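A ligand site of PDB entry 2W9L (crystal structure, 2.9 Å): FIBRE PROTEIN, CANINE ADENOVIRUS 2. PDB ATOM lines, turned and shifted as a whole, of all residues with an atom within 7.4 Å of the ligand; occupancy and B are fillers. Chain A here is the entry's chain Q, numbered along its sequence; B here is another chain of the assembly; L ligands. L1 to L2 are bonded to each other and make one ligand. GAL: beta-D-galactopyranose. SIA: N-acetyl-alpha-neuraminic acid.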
ATOM      1  N   PHE A  31      -0.180  -3.979   9.252  1.00  0.00           N
ATOM      2  CA  PHE A  31      -0.560  -2.846  10.119  1.00  0.00           C
ATOM      3  C   PHE A  31       0.211  -2.794  11.437  1.00  0.00           C
ATOM      4  O   PHE A  31       0.341  -3.809  12.126  1.00  0.00           O
ATOM      5  CB  PHE A  31      -2.045  -2.939  10.500  1.00  0.00           C
ATOM      6  CG  PHE A  31      -2.990  -2.578   9.401  1.00  0.00           C
ATOM      7  CD1 PHE A  31      -3.767  -1.436   9.485  1.00  0.00           C
ATOM      8  CD2 PHE A  31      -3.115  -3.389   8.288  1.00  0.00           C
ATOM      9  CE1 PHE A  31      -4.640  -1.105   8.477  1.00  0.00           C
ATOM     10  CE2 PHE A  31      -3.978  -3.068   7.281  1.00  0.00           C
ATOM     11  CZ  PHE A  31      -4.745  -1.928   7.366  1.00  0.00           C
ATOM     12  N   ILE A  32       0.676  -1.609  11.812  1.00  0.00           N
ATOM     13  CA  ILE A  32       1.210  -1.361  13.143  1.00  0.00           C
ATOM     14  C   ILE A  32       0.515  -0.110  13.688  1.00  0.00           C
ATOM     15  O   ILE A  32       0.790   1.011  13.251  1.00  0.00           O
ATOM     16  CB  ILE A  32       2.731  -1.187  13.105  1.00  0.00           C
ATOM     17  CG1 ILE A  32       3.380  -2.427  12.494  1.00  0.00           C
ATOM     18  CG2 ILE A  32       3.288  -0.982  14.496  1.00  0.00           C
ATOM     19  CD1 ILE A  32       4.876  -2.461  12.637  1.00  0.00           C
ATOM     20  N   ASN A  33      -0.407  -0.308  14.623  1.00  0.00           N
ATOM     21  CA  ASN A  33      -1.262   0.775  15.123  1.00  0.00           C
ATOM     22  C   ASN A  33      -2.064   1.435  13.993  1.00  0.00           C
ATOM     23  O   ASN A  33      -1.912   2.635  13.709  1.00  0.00           O
ATOM     24  CB  ASN A  33      -0.452   1.799  15.930  1.00  0.00           C
ATOM     25  CG  ASN A  33      -0.106   1.300  17.335  1.00  0.00           C
ATOM     26  OD1 ASN A  33       1.009   0.807  17.590  1.00  0.00           O
ATOM     27  ND2 ASN A  33      -1.074   1.420  18.258  1.00  0.00           N
ATOM     28  N   TYR A  63       8.533   3.167   8.387  1.00  0.00           N
ATOM     29  CA  TYR A  63       9.236   1.895   8.549  1.00  0.00           C
ATOM     30  C   TYR A  63      10.132   1.524   7.345  1.00  0.00           C
ATOM     31  O   TYR A  63      10.609   0.396   7.255  1.00  0.00           O
ATOM     32  CB  TYR A  63       8.213   0.766   8.884  1.00  0.00           C
ATOM     33  CG  TYR A  63       7.741   0.811  10.332  1.00  0.00           C
ATOM     34  CD1 TYR A  63       8.216  -0.093  11.270  1.00  0.00           C
ATOM     35  CD2 TYR A  63       6.852   1.793  10.768  1.00  0.00           C
ATOM     36  CE1 TYR A  63       7.802  -0.021  12.614  1.00  0.00           C
ATOM     37  CE2 TYR A  63       6.430   1.863  12.101  1.00  0.00           C
ATOM     38  CZ  TYR A  63       6.906   0.965  13.017  1.00  0.00           C
ATOM     39  OH  TYR A  63       6.504   1.031  14.333  1.00  0.00           O
ATOM     40  N   GLN A  70      14.718   1.041  17.319  1.00  0.00           N
ATOM     41  CA  GLN A  70      13.383   0.588  16.929  1.00  0.00           C
ATOM     42  C   GLN A  70      12.842  -0.401  17.951  1.00  0.00           C
ATOM     43  O   GLN A  70      13.526  -1.360  18.307  1.00  0.00           O
ATOM     44  CB  GLN A  70      13.429  -0.038  15.522  1.00  0.00           C
ATOM     45  CG  GLN A  70      12.148  -0.750  15.083  1.00  0.00           C
ATOM     46  CD  GLN A  70      10.966   0.182  14.965  1.00  0.00           C
ATOM     47  OE1 GLN A  70      11.017   1.178  14.257  1.00  0.00           O
ATOM     48  NE2 GLN A  70       9.868  -0.150  15.653  1.00  0.00           N
ATOM     49  N   SER A  71      11.615  -0.181  18.426  1.00  0.00           N
ATOM     50  CA  SER A  71      11.022  -1.102  19.402  1.00  0.00           C
ATOM     51  C   SER A  71      10.425  -2.312  18.680  1.00  0.00           C
ATOM     52  O   SER A  71       9.946  -2.201  17.537  1.00  0.00           O
ATOM     53  CB  SER A  71       9.975  -0.420  20.296  1.00  0.00           C
ATOM     54  OG  SER A  71       8.659  -0.665  19.827  1.00  0.00           O
ATOM     55  N   GLN A  72      10.476  -3.458  19.340  1.00  0.00           N
ATOM     56  CA  GLN A  72      10.009  -4.702  18.763  1.00  0.00           C
ATOM     57  C   GLN A  72       8.508  -4.689  18.501  1.00  0.00           C
ATOM     58  O   GLN A  72       7.778  -3.896  19.092  1.00  0.00           O
ATOM     59  CB  GLN A  72      10.375  -5.875  19.686  1.00  0.00           C
ATOM     60  CG  GLN A  72       9.549  -5.996  20.967  1.00  0.00           C
ATOM     61  CD  GLN A  72       9.727  -4.840  21.926  1.00  0.00           C
ATOM     62  OE1 GLN A  72      10.784  -4.203  21.972  1.00  0.00           O
ATOM     63  NE2 GLN A  72       8.680  -4.549  22.691  1.00  0.00           N
ATOM     64  N   PHE A  73       8.055  -5.565  17.609  1.00  0.00           N
ATOM     65  CA  PHE A  73       6.629  -5.681  17.294  1.00  0.00           C
ATOM     66  C   PHE A  73       6.207  -7.026  16.687  1.00  0.00           C
ATOM     67  O   PHE A  73       7.030  -7.761  16.120  1.00  0.00           O
ATOM     68  CB  PHE A  73       6.211  -4.560  16.338  1.00  0.00           C
ATOM     69  CG  PHE A  73       6.928  -4.581  15.018  1.00  0.00           C
ATOM     70  CD1 PHE A  73       6.390  -5.250  13.940  1.00  0.00           C
ATOM     71  CD2 PHE A  73       8.121  -3.893  14.857  1.00  0.00           C
ATOM     72  CE1 PHE A  73       7.042  -5.258  12.717  1.00  0.00           C
ATOM     73  CE2 PHE A  73       8.775  -3.883  13.620  1.00  0.00           C
ATOM     74  CZ  PHE A  73       8.235  -4.569  12.555  1.00  0.00           C
ATOM     75  N   SER A  74       4.915  -7.308  16.797  1.00  0.00           N
ATOM     76  CA  SER A  74       4.315  -8.529  16.281  1.00  0.00           C
ATOM     77  C   SER A  74       3.347  -8.233  15.153  1.00  0.00           C
ATOM     78  O   SER A  74       2.534  -7.314  15.237  1.00  0.00           O
ATOM     79  CB  SER A  74       3.568  -9.249  17.395  1.00  0.00           C
ATOM     80  OG  SER A  74       4.440 -10.090  18.134  1.00  0.00           O
ATOM     81  N   LEU A  75       3.442  -9.021  14.095  1.00  0.00           N
ATOM     82  CA  LEU A  75       2.437  -9.024  13.043  1.00  0.00           C
ATOM     83  C   LEU A  75       1.685 -10.355  13.132  1.00  0.00           C
ATOM     84  O   LEU A  75       2.234 -11.398  12.765  1.00  0.00           O
ATOM     85  CB  LEU A  75       3.133  -8.804  11.696  1.00  0.00           C
ATOM     86  CG  LEU A  75       3.888  -7.458  11.584  1.00  0.00           C
ATOM     87  CD1 LEU A  75       4.552  -7.256  10.229  1.00  0.00           C
ATOM     88  CD2 LEU A  75       2.960  -6.312  11.844  1.00  0.00           C
ATOM     89  N   ILE A  76       0.462 -10.318  13.663  1.00  0.00           N
ATOM     90  CA  ILE A  76      -0.312 -11.521  13.931  1.00  0.00           C
ATOM     91  C   ILE A  76      -1.331 -11.766  12.833  1.00  0.00           C
ATOM     92  O   ILE A  76      -2.088 -10.855  12.462  1.00  0.00           O
ATOM     93  CB  ILE A  76      -1.037 -11.439  15.300  1.00  0.00           C
ATOM     94  CG1 ILE A  76      -0.032 -11.085  16.428  1.00  0.00           C
ATOM     95  CG2 ILE A  76      -1.760 -12.752  15.602  1.00  0.00           C
ATOM     96  CD1 ILE A  76      -0.664 -10.468  17.699  1.00  0.00           C
ATOM     97  N   ASN A  90      -3.049  -8.199  12.544  1.00  0.00           N
ATOM     98  CA  ASN A  90      -2.206  -7.173  11.905  1.00  0.00           C
ATOM     99  C   ASN A  90      -2.126  -7.389  10.411  1.00  0.00           C
ATOM    100  O   ASN A  90      -1.955  -6.454   9.649  1.00  0.00           O
ATOM    101  CB  ASN A  90      -0.773  -7.198  12.452  1.00  0.00           C
ATOM    102  CG  ASN A  90      -0.678  -6.798  13.918  1.00  0.00           C
ATOM    103  OD1 ASN A  90      -0.809  -7.627  14.825  1.00  0.00           O
ATOM    104  ND2 ASN A  90      -0.410  -5.518  14.164  1.00  0.00           N
ATOM    105  N   LYS A 158      -0.311 -18.826  19.386  1.00  0.00           N
ATOM    106  CA  LYS A 158      -0.485 -18.044  20.594  1.00  0.00           C
ATOM    107  C   LYS A 158      -1.923 -17.533  20.566  1.00  0.00           C
ATOM    108  O   LYS A 158      -2.371 -17.025  19.542  1.00  0.00           O
ATOM    109  CB  LYS A 158       0.504 -16.888  20.711  1.00  0.00           C
ATOM    110  CG  LYS A 158       0.689 -16.510  22.155  1.00  0.00           C
ATOM    111  CD  LYS A 158       1.587 -15.299  22.360  1.00  0.00           C
ATOM    112  CE  LYS A 158       1.574 -14.870  23.826  1.00  0.00           C
ATOM    113  NZ  LYS A 158       1.879 -13.442  23.953  1.00  0.00           N
ATOM    114  N   LYS A 160      -5.179 -15.411  20.608  1.00  0.00           N
ATOM    115  CA  LYS A 160      -5.486 -14.006  20.346  1.00  0.00           C
ATOM    116  C   LYS A 160      -6.972 -13.892  19.974  1.00  0.00           C
ATOM    117  O   LYS A 160      -7.444 -14.514  19.013  1.00  0.00           O
ATOM    118  CB  LYS A 160      -4.580 -13.472  19.234  1.00  0.00           C
ATOM    119  CG  LYS A 160      -4.748 -11.998  18.914  1.00  0.00           C
ATOM    120  CD  LYS A 160      -4.484 -11.105  20.140  1.00  0.00           C
ATOM    121  CE  LYS A 160      -4.018  -9.688  19.737  1.00  0.00           C
ATOM    122  NZ  LYS A 160      -4.917  -9.032  18.706  1.00  0.00           N
ATOM    123  N   THR A 168       2.323 -15.667  14.147  1.00  0.00           N
ATOM    124  CA  THR A 168       2.856 -14.367  14.512  1.00  0.00           C
ATOM    125  C   THR A 168       4.279 -14.239  14.020  1.00  0.00           C
ATOM    126  O   THR A 168       5.146 -15.051  14.366  1.00  0.00           O
ATOM    127  CB  THR A 168       2.864 -14.150  16.051  1.00  0.00           C
ATOM    128  OG1 THR A 168       1.544 -14.364  16.564  1.00  0.00           O
ATOM    129  CG2 THR A 168       3.326 -12.730  16.421  1.00  0.00           C
ATOM    130  N   PHE A 169       4.529 -13.218  13.204  1.00  0.00           N
ATOM    131  CA  PHE A 169       5.892 -12.819  12.881  1.00  0.00           C
ATOM    132  C   PHE A 169       6.258 -11.698  13.844  1.00  0.00           C
ATOM    133  O   PHE A 169       5.663 -10.637  13.798  1.00  0.00           O
ATOM    134  CB  PHE A 169       6.017 -12.378  11.426  1.00  0.00           C
ATOM    135  CG  PHE A 169       5.556 -13.421  10.454  1.00  0.00           C
ATOM    136  CD1 PHE A 169       6.415 -14.400  10.017  1.00  0.00           C
ATOM    137  CD2 PHE A 169       4.235 -13.436  10.012  1.00  0.00           C
ATOM    138  CE1 PHE A 169       5.984 -15.378   9.135  1.00  0.00           C
ATOM    139  CE2 PHE A 169       3.796 -14.407   9.109  1.00  0.00           C
ATOM    140  CZ  PHE A 169       4.665 -15.376   8.680  1.00  0.00           C
ATOM    141  N   ARG A 170       7.210 -11.985  14.746  1.00  0.00           N
ATOM    142  CA  ARG A 170       7.611 -11.030  15.763  1.00  0.00           C
ATOM    143  C   ARG A 170       9.051 -10.614  15.511  1.00  0.00           C
ATOM    144  O   ARG A 170       9.945 -11.450  15.527  1.00  0.00           O
ATOM    145  CB  ARG A 170       7.488 -11.646  17.159  1.00  0.00           C
ATOM    146  CG  ARG A 170       7.726 -10.650  18.273  1.00  0.00           C
ATOM    147  CD  ARG A 170       7.116 -11.108  19.588  1.00  0.00           C
ATOM    148  NE  ARG A 170       7.396 -10.215  20.713  1.00  0.00           N
ATOM    149  CZ  ARG A 170       6.794  -9.041  20.941  1.00  0.00           C
ATOM    150  NH1 ARG A 170       5.869  -8.579  20.119  1.00  0.00           N
ATOM    151  NH2 ARG A 170       7.146  -8.322  21.990  1.00  0.00           N
ATOM    152  N   LEU A 172      12.450  -8.666  16.438  1.00  0.00           N
ATOM    153  CA  LEU A 172      13.097  -8.427  17.725  1.00  0.00           C
ATOM    154  C   LEU A 172      14.567  -8.064  17.577  1.00  0.00           C
ATOM    155  O   LEU A 172      15.201  -8.311  16.541  1.00  0.00           O
ATOM    156  CB  LEU A 172      13.028  -9.688  18.585  1.00  0.00           C
ATOM    157  CG  LEU A 172      11.688 -10.176  19.099  1.00  0.00           C
ATOM    158  CD1 LEU A 172      11.665 -11.713  19.168  1.00  0.00           C
ATOM    159  CD2 LEU A 172      11.375  -9.551  20.444  1.00  0.00           C
ATOM    160  N   PHE A 174      16.390  -5.254  17.465  1.00  0.00           N
ATOM    161  CA  PHE A 174      16.878  -4.233  16.537  1.00  0.00           C
ATOM    162  C   PHE A 174      18.171  -3.597  17.012  1.00  0.00           C
ATOM    163  O   PHE A 174      18.965  -3.110  16.199  1.00  0.00           O
ATOM    164  CB  PHE A 174      15.823  -3.134  16.332  1.00  0.00           C
ATOM    165  CG  PHE A 174      14.677  -3.547  15.484  1.00  0.00           C
ATOM    166  CD1 PHE A 174      14.693  -3.293  14.122  1.00  0.00           C
ATOM    167  CD2 PHE A 174      13.585  -4.202  16.031  1.00  0.00           C
ATOM    168  CE1 PHE A 174      13.626  -3.681  13.334  1.00  0.00           C
ATOM    169  CE2 PHE A 174      12.508  -4.600  15.234  1.00  0.00           C
ATOM    170  CZ  PHE A 174      12.523  -4.331  13.900  1.00  0.00           C
ATOM    171  N   ASP B 143      10.973 -13.650  25.511  1.00  0.00           N
ATOM    172  CA  ASP B 143      10.830 -12.782  24.361  1.00  0.00           C
ATOM    173  C   ASP B 143      12.067 -12.766  23.464  1.00  0.00           C
ATOM    174  O   ASP B 143      12.548 -11.710  23.048  1.00  0.00           O
ATOM    175  CB  ASP B 143      10.435 -11.377  24.767  1.00  0.00           C
ATOM    176  CG  ASP B 143       9.622 -10.685  23.692  1.00  0.00           C
ATOM    177  OD1 ASP B 143       8.796 -11.384  23.036  1.00  0.00           O
ATOM    178  OD2 ASP B 143       9.790  -9.472  23.488  1.00  0.00           O
HETATM  179  C1  GAL L   1      -0.071  -6.184  24.242  1.00  0.00           C
HETATM  180  C2  GAL L   1       1.185  -6.215  23.324  1.00  0.00           C
HETATM  181  C3  GAL L   1       1.829  -4.828  23.270  1.00  0.00           C
HETATM  182  C4  GAL L   1       0.859  -3.691  23.031  1.00  0.00           C
HETATM  183  C5  GAL L   1      -0.060  -3.776  24.240  1.00  0.00           C
HETATM  184  C6  GAL L   1      -0.927  -2.546  24.435  1.00  0.00           C
HETATM  185  O1  GAL L   1      -0.913  -7.330  24.027  1.00  0.00           O
HETATM  186  O2  GAL L   1       2.111  -7.146  23.879  1.00  0.00           O
HETATM  187  O3  GAL L   1       3.235  -4.557  23.423  1.00  0.00           O
HETATM  188  O4  GAL L   1       0.113  -3.870  21.809  1.00  0.00           O
HETATM  189  O5  GAL L   1      -0.838  -4.968  24.078  1.00  0.00           O
HETATM  190  O6  GAL L   1      -0.795  -2.127  25.798  1.00  0.00           O
HETATM  191  C1  SIA L   2       4.913  -5.311  21.938  1.00  0.00           C
HETATM  192  C2  SIA L   2       4.053  -4.132  22.297  1.00  0.00           C
HETATM  193  C3  SIA L   2       4.955  -2.971  22.725  1.00  0.00           C
HETATM  194  C4  SIA L   2       5.838  -2.483  21.580  1.00  0.00           C
HETATM  195  C5  SIA L   2       4.953  -2.026  20.424  1.00  0.00           C
HETATM  196  C6  SIA L   2       4.175  -3.263  20.016  1.00  0.00           C
HETATM  197  C7  SIA L   2       3.335  -3.093  18.765  1.00  0.00           C
HETATM  198  C8  SIA L   2       2.461  -4.321  18.472  1.00  0.00           C
HETATM  199  C9  SIA L   2       2.012  -4.323  17.016  1.00  0.00           C
HETATM  200  C10 SIA L   2       5.622  -0.772  18.369  1.00  0.00           C
HETATM  201  C11 SIA L   2       6.746  -0.590  17.385  1.00  0.00           C
HETATM  202  N5  SIA L   2       5.855  -1.648  19.352  1.00  0.00           N
HETATM  203  O1A SIA L   2       4.564  -6.041  20.993  1.00  0.00           O
HETATM  204  O1B SIA L   2       5.946  -5.505  22.602  1.00  0.00           O
HETATM  205  O4  SIA L   2       6.710  -1.451  22.022  1.00  0.00           O
HETATM  206  O6  SIA L   2       3.348  -3.692  21.122  1.00  0.00           O
HETATM  207  O7  SIA L   2       2.525  -1.936  18.915  1.00  0.00           O
HETATM  208  O8  SIA L   2       3.144  -5.548  18.706  1.00  0.00           O
HETATM  209  O9  SIA L   2       1.487  -5.606  16.699  1.00  0.00           O
HETATM  210  O10 SIA L   2       4.587  -0.157  18.257  1.00  0.00           O
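The backbone NH of Ser 74 is in hydrogen-bond range of an oxygen (O8) of SIA L2 (3.1 Å).
The backbone carbonyl oxygen (O) of Ser 74 lies within hydrogen-bond range of an oxygen (O9) of SIA L2, 2.5 Å away.
O of Gln 72 is in hydrogen-bond range of N5 of SIA L2, 3.0 Å away.
The side-chain amide nitrogen (NE2) of Gln 72 sits at hydrogen-bond distance from an oxygen (O1B) of SIA L2, 2.9 Å away.
NH1 of Arg 170 lies within salt-bridge range of O1A of SIA L2 (3.0 Å).
The side-chain hydroxyl (OG) of Ser 71 is in hydrogen-bond range of a nitrogen (N5) of SIA L2 (3.0 Å).
The side-chain amide nitrogen of Asn 90 sits at hydrogen-bond distance from an oxygen (O9) of SIA L2 (3.2 Å).
OD1 of Asn 33 is in hydrogen-bond range of O7 of SIA L2 (3.4 Å).
Residues that only touch the ligand: Tyr 63, Gln 70 and Phe 73.
Hydrophobic or aromatic side chains within 4 Å of the ligand: Phe 73.
Of the 20 residues printed, 9 come within 4 Å of the ligand.
The nearest printed residue that does not touch the ligand is Ile 32 (4.1 Å).
The guanidinium group (NH1) of Arg 170 is in hydrogen-bond range of the side-chain hydroxyl (OG) of Ser 74 (2.9 Å).
The backbone carbonyl oxygen of Ser 74 lies close to the side-chain amide oxygen of Asn 90 (3.4 Å).
The guanidinium group (NE) of Arg 170 lies within salt-bridge range of the side-chain carboxylate (OD1) of Asp 143 of chain B (3.0 Å).
The side-chain amide nitrogen (ND2) of Asn 90 lies within hydrogen-bond range of the backbone carbonyl oxygen (O) of Phe 31, 2.8 Å away.
O of Ile 76 is in hydrogen-bond range of N of Asn 90.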
